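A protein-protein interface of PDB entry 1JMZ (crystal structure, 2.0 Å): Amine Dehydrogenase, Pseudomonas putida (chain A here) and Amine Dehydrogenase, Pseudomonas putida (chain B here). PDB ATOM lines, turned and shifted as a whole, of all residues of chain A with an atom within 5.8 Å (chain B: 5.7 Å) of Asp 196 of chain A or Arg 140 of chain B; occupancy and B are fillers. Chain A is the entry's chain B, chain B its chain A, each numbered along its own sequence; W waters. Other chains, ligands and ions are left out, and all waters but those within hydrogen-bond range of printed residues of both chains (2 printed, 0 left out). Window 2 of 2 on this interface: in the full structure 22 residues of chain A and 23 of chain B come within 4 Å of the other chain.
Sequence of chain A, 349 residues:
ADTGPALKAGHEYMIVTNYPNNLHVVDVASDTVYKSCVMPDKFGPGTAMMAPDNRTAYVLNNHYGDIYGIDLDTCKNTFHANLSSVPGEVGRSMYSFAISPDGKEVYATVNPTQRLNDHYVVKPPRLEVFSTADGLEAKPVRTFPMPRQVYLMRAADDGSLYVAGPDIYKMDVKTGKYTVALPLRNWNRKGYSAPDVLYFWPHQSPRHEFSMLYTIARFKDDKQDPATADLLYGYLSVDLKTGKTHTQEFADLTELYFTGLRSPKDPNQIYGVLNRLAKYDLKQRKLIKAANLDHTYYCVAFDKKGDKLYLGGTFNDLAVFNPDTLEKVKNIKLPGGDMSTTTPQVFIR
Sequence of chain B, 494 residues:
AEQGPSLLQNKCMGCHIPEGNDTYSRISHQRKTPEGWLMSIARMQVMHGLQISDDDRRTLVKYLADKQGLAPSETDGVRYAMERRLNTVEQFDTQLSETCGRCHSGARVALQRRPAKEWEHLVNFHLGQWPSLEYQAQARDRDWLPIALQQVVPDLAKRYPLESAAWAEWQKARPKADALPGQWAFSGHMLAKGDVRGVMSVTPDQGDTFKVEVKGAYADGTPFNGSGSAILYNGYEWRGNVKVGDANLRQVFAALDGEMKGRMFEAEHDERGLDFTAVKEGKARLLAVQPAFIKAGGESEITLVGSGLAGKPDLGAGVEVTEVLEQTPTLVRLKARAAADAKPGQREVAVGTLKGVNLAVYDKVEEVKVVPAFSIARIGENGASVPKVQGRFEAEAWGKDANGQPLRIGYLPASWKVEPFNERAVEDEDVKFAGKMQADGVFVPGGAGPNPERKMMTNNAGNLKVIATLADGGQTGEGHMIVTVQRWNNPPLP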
ATOM      1  N   GLN A 149     -30.355  29.963  24.537  1.00  0.00           N
ATOM      2  CA  GLN A 149     -30.595  29.649  23.134  1.00  0.00           C
ATOM      3  C   GLN A 149     -31.974  29.086  22.789  1.00  0.00           C
ATOM      4  O   GLN A 149     -32.136  28.324  21.834  1.00  0.00           O
ATOM      5  CB  GLN A 149     -29.466  28.772  22.591  1.00  0.00           C
ATOM      6  CG  GLN A 149     -28.098  29.444  22.652  1.00  0.00           C
ATOM      7  CD  GLN A 149     -26.949  28.467  22.473  1.00  0.00           C
ATOM      8  OE1 GLN A 149     -26.921  27.401  23.096  1.00  0.00           O
ATOM      9  NE2 GLN A 149     -25.978  28.838  21.646  1.00  0.00           N
ATOM     10  N   ARG A 185     -29.278  18.756  19.949  1.00  0.00           N
ATOM     11  CA  ARG A 185     -27.864  18.889  20.248  1.00  0.00           C
ATOM     12  C   ARG A 185     -27.315  17.630  20.911  1.00  0.00           C
ATOM     13  O   ARG A 185     -26.200  17.196  20.607  1.00  0.00           O
ATOM     14  CB  ARG A 185     -27.581  20.092  21.142  1.00  0.00           C
ATOM     15  CG  ARG A 185     -26.083  20.273  21.360  1.00  0.00           C
ATOM     16  CD  ARG A 185     -25.756  21.494  22.147  1.00  0.00           C
ATOM     17  NE  ARG A 185     -26.200  22.716  21.496  1.00  0.00           N
ATOM     18  CZ  ARG A 185     -26.068  23.914  22.047  1.00  0.00           C
ATOM     19  NH1 ARG A 185     -25.500  24.020  23.227  1.00  0.00           N
ATOM     20  NH2 ARG A 185     -26.575  24.990  21.467  1.00  0.00           N
ATOM     21  N   ALA A 194     -24.507  16.256  14.761  1.00  0.00           N
ATOM     22  CA  ALA A 194     -25.631  16.824  15.486  1.00  0.00           C
ATOM     23  C   ALA A 194     -26.400  17.632  14.439  1.00  0.00           C
ATOM     24  O   ALA A 194     -25.796  18.151  13.490  1.00  0.00           O
ATOM     25  CB  ALA A 194     -25.130  17.751  16.593  1.00  0.00           C
ATOM     26  N   PRO A 195     -27.741  17.701  14.553  1.00  0.00           N
ATOM     27  CA  PRO A 195     -28.492  18.479  13.557  1.00  0.00           C
ATOM     28  C   PRO A 195     -28.344  19.994  13.759  1.00  0.00           C
ATOM     29  O   PRO A 195     -27.946  20.460  14.831  1.00  0.00           O
ATOM     30  CB  PRO A 195     -29.933  18.011  13.778  1.00  0.00           C
ATOM     31  CG  PRO A 195     -29.960  17.671  15.231  1.00  0.00           C
ATOM     32  CD  PRO A 195     -28.650  16.968  15.454  1.00  0.00           C
ATOM     33  N   ASP A 196     -28.582  20.748  12.693  1.00  0.00           N
ATOM     34  CA  ASP A 196     -28.517  22.201  12.761  1.00  0.00           C
ATOM     35  C   ASP A 196     -29.929  22.693  12.462  1.00  0.00           C
ATOM     36  O   ASP A 196     -30.560  22.252  11.502  1.00  0.00           O
ATOM     37  CB  ASP A 196     -27.516  22.769  11.748  1.00  0.00           C
ATOM     38  CG  ASP A 196     -27.292  24.259  11.935  1.00  0.00           C
ATOM     39  OD1 ASP A 196     -26.559  24.641  12.862  1.00  0.00           O
ATOM     40  OD2 ASP A 196     -27.859  25.056  11.171  1.00  0.00           O
ATOM     41  N   VAL A 197     -30.446  23.561  13.323  1.00  0.00           N
ATOM     42  CA  VAL A 197     -31.791  24.080  13.143  1.00  0.00           C
ATOM     43  C   VAL A 197     -31.821  25.594  13.249  1.00  0.00           C
ATOM     44  O   VAL A 197     -31.461  26.168  14.278  1.00  0.00           O
ATOM     45  CB  VAL A 197     -32.789  23.510  14.192  1.00  0.00           C
ATOM     46  CG1 VAL A 197     -34.208  23.917  13.838  1.00  0.00           C
ATOM     47  CG2 VAL A 197     -32.680  21.999  14.287  1.00  0.00           C
ATOM     48  N   LEU A 198     -32.259  26.222  12.163  1.00  0.00           N
ATOM     49  CA  LEU A 198     -32.404  27.668  12.071  1.00  0.00           C
ATOM     50  C   LEU A 198     -33.861  27.847  11.633  1.00  0.00           C
ATOM     51  O   LEU A 198     -34.188  27.699  10.459  1.00  0.00           O
ATOM     52  CB  LEU A 198     -31.427  28.230  11.020  1.00  0.00           C
ATOM     53  CG  LEU A 198     -31.259  29.750  10.854  1.00  0.00           C
ATOM     54  CD1 LEU A 198     -32.360  30.323   9.961  1.00  0.00           C
ATOM     55  CD2 LEU A 198     -31.221  30.442  12.229  1.00  0.00           C
ATOM     56  N   LEU A 213     -37.551  22.385   9.968  1.00  0.00           N
ATOM     57  CA  LEU A 213     -36.633  21.670   9.091  1.00  0.00           C
ATOM     58  C   LEU A 213     -35.269  21.753   9.767  1.00  0.00           C
ATOM     59  O   LEU A 213     -35.017  22.656  10.574  1.00  0.00           O
ATOM     60  CB  LEU A 213     -36.524  22.334   7.717  1.00  0.00           C
ATOM     61  CG  LEU A 213     -37.698  22.458   6.749  1.00  0.00           C
ATOM     62  CD1 LEU A 213     -37.172  23.140   5.489  1.00  0.00           C
ATOM     63  CD2 LEU A 213     -38.305  21.103   6.422  1.00  0.00           C
ATOM     64  N   TYR A 214     -34.415  20.783   9.476  1.00  0.00           N
ATOM     65  CA  TYR A 214     -33.059  20.760  10.009  1.00  0.00           C
ATOM     66  C   TYR A 214     -32.157  20.111   8.972  1.00  0.00           C
ATOM     67  O   TYR A 214     -32.638  19.487   8.027  1.00  0.00           O
ATOM     68  CB  TYR A 214     -32.976  19.980  11.332  1.00  0.00           C
ATOM     69  CG  TYR A 214     -33.321  18.506  11.240  1.00  0.00           C
ATOM     70  CD1 TYR A 214     -32.337  17.552  10.984  1.00  0.00           C
ATOM     71  CD2 TYR A 214     -34.635  18.068  11.422  1.00  0.00           C
ATOM     72  CE1 TYR A 214     -32.652  16.197  10.912  1.00  0.00           C
ATOM     73  CE2 TYR A 214     -34.964  16.711  11.353  1.00  0.00           C
ATOM     74  CZ  TYR A 214     -33.967  15.784  11.097  1.00  0.00           C
ATOM     75  OH  TYR A 214     -34.289  14.452  11.030  1.00  0.00           O
ATOM     76  N   THR A 215     -30.854  20.337   9.100  1.00  0.00           N
ATOM     77  CA  THR A 215     -29.891  19.719   8.208  1.00  0.00           C
ATOM     78  C   THR A 215     -29.034  18.859   9.113  1.00  0.00           C
ATOM     79  O   THR A 215     -28.982  19.087  10.323  1.00  0.00           O
ATOM     80  CB  THR A 215     -29.014  20.746   7.468  1.00  0.00           C
ATOM     81  OG1 THR A 215     -28.315  21.564   8.415  1.00  0.00           O
ATOM     82  CG2 THR A 215     -29.859  21.612   6.553  1.00  0.00           C
ATOM     83  N   ILE A 216     -28.405  17.838   8.546  1.00  0.00           N
ATOM     84  CA  ILE A 216     -27.558  16.950   9.332  1.00  0.00           C
ATOM     85  C   ILE A 216     -26.602  16.219   8.401  1.00  0.00           C
ATOM     86  O   ILE A 216     -26.961  15.865   7.279  1.00  0.00           O
ATOM     87  CB  ILE A 216     -28.411  15.944  10.163  1.00  0.00           C
ATOM     88  CG1 ILE A 216     -27.533  15.214  11.181  1.00  0.00           C
ATOM     89  CG2 ILE A 216     -29.145  14.971   9.242  1.00  0.00           C
ATOM     90  CD1 ILE A 216     -28.273  14.247  12.056  1.00  0.00           C
ATOM     91  N   LEU B 133     -26.748  36.905  18.553  1.00  0.00           N
ATOM     92  CA  LEU B 133     -25.393  36.365  18.459  1.00  0.00           C
ATOM     93  C   LEU B 133     -25.273  34.859  18.715  1.00  0.00           C
ATOM     94  O   LEU B 133     -24.678  34.141  17.913  1.00  0.00           O
ATOM     95  CB  LEU B 133     -24.459  37.138  19.412  1.00  0.00           C
ATOM     96  CG  LEU B 133     -22.938  36.919  19.441  1.00  0.00           C
ATOM     97  CD1 LEU B 133     -22.265  38.123  20.063  1.00  0.00           C
ATOM     98  CD2 LEU B 133     -22.562  35.662  20.203  1.00  0.00           C
ATOM     99  N   GLU B 134     -25.837  34.396  19.830  1.00  0.00           N
ATOM    100  CA  GLU B 134     -25.767  32.987  20.229  1.00  0.00           C
ATOM    101  C   GLU B 134     -26.695  32.030  19.480  1.00  0.00           C
ATOM    102  O   GLU B 134     -26.736  30.843  19.783  1.00  0.00           O
ATOM    103  CB  GLU B 134     -25.989  32.861  21.740  1.00  0.00           C
ATOM    104  CG  GLU B 134     -27.369  33.292  22.190  1.00  0.00           C
ATOM    105  CD  GLU B 134     -27.528  33.339  23.698  1.00  0.00           C
ATOM    106  OE1 GLU B 134     -26.865  32.558  24.413  1.00  0.00           O
ATOM    107  OE2 GLU B 134     -28.331  34.163  24.168  1.00  0.00           O
ATOM    108  N   TYR B 135     -27.447  32.551  18.518  1.00  0.00           N
ATOM    109  CA  TYR B 135     -28.359  31.744  17.716  1.00  0.00           C
ATOM    110  C   TYR B 135     -27.857  31.657  16.281  1.00  0.00           C
ATOM    111  O   TYR B 135     -28.508  31.061  15.432  1.00  0.00           O
ATOM    112  CB  TYR B 135     -29.754  32.364  17.697  1.00  0.00           C
ATOM    113  CG  TYR B 135     -30.457  32.400  19.028  1.00  0.00           C
ATOM    114  CD1 TYR B 135     -31.381  31.413  19.369  1.00  0.00           C
ATOM    115  CD2 TYR B 135     -30.237  33.441  19.931  1.00  0.00           C
ATOM    116  CE1 TYR B 135     -32.069  31.463  20.566  1.00  0.00           C
ATOM    117  CE2 TYR B 135     -30.922  33.496  21.136  1.00  0.00           C
ATOM    118  CZ  TYR B 135     -31.837  32.503  21.444  1.00  0.00           C
ATOM    119  OH  TYR B 135     -32.524  32.540  22.624  1.00  0.00           O
ATOM    120  N   GLN B 136     -26.724  32.307  16.024  1.00  0.00           N
ATOM    121  CA  GLN B 136     -26.101  32.353  14.703  1.00  0.00           C
ATOM    122  C   GLN B 136     -25.154  31.187  14.476  1.00  0.00           C
ATOM    123  O   GLN B 136     -24.812  30.470  15.409  1.00  0.00           O
ATOM    124  CB  GLN B 136     -25.338  33.674  14.535  1.00  0.00           C
ATOM    125  CG  GLN B 136     -26.222  34.905  14.508  1.00  0.00           C
ATOM    126  CD  GLN B 136     -25.442  36.197  14.609  1.00  0.00           C
ATOM    127  OE1 GLN B 136     -24.223  36.211  14.488  1.00  0.00           O
ATOM    128  NE2 GLN B 136     -26.147  37.295  14.849  1.00  0.00           N
ATOM    129  N   ALA B 137     -24.724  31.015  13.227  1.00  0.00           N
ATOM    130  CA  ALA B 137     -23.802  29.943  12.862  1.00  0.00           C
ATOM    131  C   ALA B 137     -22.545  30.044  13.711  1.00  0.00           C
ATOM    132  O   ALA B 137     -22.072  31.148  13.998  1.00  0.00           O
ATOM    133  CB  ALA B 137     -23.447  30.034  11.386  1.00  0.00           C
ATOM    134  N   GLN B 138     -22.021  28.886  14.112  1.00  0.00           N
ATOM    135  CA  GLN B 138     -20.829  28.776  14.956  1.00  0.00           C
ATOM    136  C   GLN B 138     -21.085  29.314  16.371  1.00  0.00           C
ATOM    137  O   GLN B 138     -20.151  29.610  17.114  1.00  0.00           O
ATOM    138  CB  GLN B 138     -19.617  29.463  14.320  1.00  0.00           C
ATOM    139  CG  GLN B 138     -19.103  28.822  13.036  1.00  0.00           C
ATOM    140  CD  GLN B 138     -18.157  29.745  12.275  1.00  0.00           C
ATOM    141  OE1 GLN B 138     -18.589  30.653  11.561  1.00  0.00           O
ATOM    142  NE2 GLN B 138     -16.861  29.528  12.441  1.00  0.00           N
ATOM    143  N   ALA B 139     -22.361  29.426  16.727  1.00  0.00           N
ATOM    144  CA  ALA B 139     -22.774  29.879  18.048  1.00  0.00           C
ATOM    145  C   ALA B 139     -23.892  28.972  18.581  1.00  0.00           C
ATOM    146  O   ALA B 139     -23.816  28.500  19.708  1.00  0.00           O
ATOM    147  CB  ALA B 139     -23.237  31.325  17.996  1.00  0.00           C
ATOM    148  N   ARG B 140     -24.894  28.695  17.743  1.00  0.00           N
ATOM    149  CA  ARG B 140     -26.041  27.843  18.107  1.00  0.00           C
ATOM    150  C   ARG B 140     -25.667  26.367  18.285  1.00  0.00           C
ATOM    151  O   ARG B 140     -26.473  25.572  18.758  1.00  0.00           O
ATOM    152  CB  ARG B 140     -27.136  27.932  17.033  1.00  0.00           C
ATOM    153  CG  ARG B 140     -26.880  27.028  15.828  1.00  0.00           C
ATOM    154  CD  ARG B 140     -27.973  27.105  14.800  1.00  0.00           C
ATOM    155  NE  ARG B 140     -27.950  28.408  14.173  1.00  0.00           N
ATOM    156  CZ  ARG B 140     -27.809  28.639  12.873  1.00  0.00           C
ATOM    157  NH1 ARG B 140     -27.687  27.646  12.009  1.00  0.00           N
ATOM    158  NH2 ARG B 140     -27.739  29.890  12.453  1.00  0.00           N
ATOM    159  N   ASP B 141     -24.482  25.995  17.817  1.00  0.00           N
ATOM    160  CA  ASP B 141     -23.996  24.626  17.914  1.00  0.00           C
ATOM    161  C   ASP B 141     -23.241  24.346  19.207  1.00  0.00           C
ATOM    162  O   ASP B 141     -22.777  23.226  19.426  1.00  0.00           O
ATOM    163  CB  ASP B 141     -23.101  24.300  16.712  1.00  0.00           C
ATOM    164  CG  ASP B 141     -21.842  25.168  16.641  1.00  0.00           C
ATOM    165  OD1 ASP B 141     -21.756  26.234  17.297  1.00  0.00           O
ATOM    166  OD2 ASP B 141     -20.925  24.780  15.894  1.00  0.00           O
ATOM    167  N   ARG B 142     -23.148  25.355  20.072  1.00  0.00           N
ATOM    168  CA  ARG B 142     -22.424  25.226  21.336  1.00  0.00           C
ATOM    169  C   ARG B 142     -23.009  26.128  22.432  1.00  0.00           C
ATOM    170  O   ARG B 142     -23.960  26.870  22.194  1.00  0.00           O
ATOM    171  CB  ARG B 142     -20.955  25.605  21.112  1.00  0.00           C
ATOM    172  CG  ARG B 142     -20.723  27.101  20.860  1.00  0.00           C
ATOM    173  CD  ARG B 142     -19.383  27.381  20.190  1.00  0.00           C
ATOM    174  NE  ARG B 142     -19.362  26.873  18.822  1.00  0.00           N
ATOM    175  CZ  ARG B 142     -18.348  27.005  17.974  1.00  0.00           C
ATOM    176  NH1 ARG B 142     -17.246  27.636  18.342  1.00  0.00           N
ATOM    177  NH2 ARG B 142     -18.444  26.499  16.752  1.00  0.00           N
HETATM  178  O   HOH W   1     -33.147  31.615  25.699  1.00  0.00           O
HETATM  179  O   HOH W   2     -30.326  32.814  25.583  1.00  0.00           O
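The side-chain amide nitrogen (NE2) of Gln 149 of chain A sits at hydrogen-bond distance from the backbone carbonyl oxygen (O) of Glu 134 of chain B, 2.8 Å away.
NE2 of Gln 149 of chain A sits at hydrogen-bond distance from O of Ala 139 of chain B (2.9 Å).
The backbone carbonyl oxygen (O) of Arg 140 of chain B is in hydrogen-bond range of the guanidinium group (NH2) of Arg 185 of chain A.
The guanidinium group (NH1) of Arg 140 of chain B lies within salt-bridge range of the side-chain carboxylate (OD2) of Asp 196 of chain A, 2.7 Å away.
O of Arg 142 of chain B lies within hydrogen-bond range of NE2 of Gln 149 of chain A (2.9 Å).
O of Arg 142 of chain B is in hydrogen-bond range of NH2 of Arg 185 of chain A (3.3 Å).
N of Arg 140 of chain B is in hydrogen-bond range of O of Glu 134 of chain B, 3.5 Å away.
The backbone carbonyl oxygen (O) of Tyr 135 of chain B is in hydrogen-bond range of the guanidinium group (NE) of Arg 140 of chain B, at 3.0 Å.
The guanidinium group of Arg 142 of chain B lies close to the backbone carbonyl oxygen of Gln 138 of chain B, 3.3 Å away.
The backbone NH of Ala 139 of chain B sits at hydrogen-bond distance from the side-chain carboxylate of Asp 141 of chain B (3.3 Å).
OD1 of Asp 141 of chain B is in salt-bridge range of NE of Arg 142 of chain B (2.9 Å).
N of Asp 196 of chain A lies within hydrogen-bond range of O of Thr 215 of chain A, 2.9 Å away.
Gln 149 of chain A touches Tyr 135 of chain B (C to CE1, 3.3 Å).
Arg 140 of chain B touches Gln 149 of chain A (CA to NE2, 3.7 Å).
Val 197 of chain A touches Arg 140 of chain B (O to CD, 3.6 Å).
CD2 of Leu 198 of chain A touches NH2 of Arg 140 of chain B, at 3.5 Å.
Of the printed residues of chain B, Asp 196 of chain A touches Arg 140 (2.7 Å).
Printed residues of chain A within 4 Å of Arg 140 of chain B: Gln 149 (3.7 Å), Arg 185 (2.8 Å), Asp 196 (2.7 Å), Val 197 (3.6 Å) and Leu 198 (3.5 Å).
Of the printed residues of chain A, Ala 139 of chain B touches Gln 149.
Of the printed residues of chain A, Tyr 135 of chain B touches Gln 149 (3.3 Å).
Thr 215 of chain A touches none of the printed residues of chain B.
Ile 216 of chain A touches none of the printed residues of chain B.
The nearest residue of chain B that does not touch Asp 196 of chain A is Asp 141 of chain B (5.2 Å).
The nearest printed residue of chain A that does not touch Arg 140 of chain B is Pro 195 of chain A (6.6 Å).
Hydrophobic or aromatic side chains of chain A within 4 Å of the printed part of chain B: Leu 198.
Hydrophobic or aromatic side chains of chain B within 4 Å of the printed part of chain A: Tyr 135.
Among the printed residues, 10 pairs touch across the chains.
Among the printed residues, Asp or Glu carboxylates within 4 Å of a Lys or Arg side-chain nitrogen of the other chain: Asp 196 of chain A with Arg 140 of chain B.
Water W2 bridges the side-chain carboxylate (OE2) of Glu 134 of chain B and the backbone NH (N) of Gln 149 of chain A.
Water W1 bridges OH of Tyr 135 of chain B (3.3 Å) and N of Gln 149 of chain A (3.4 Å).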
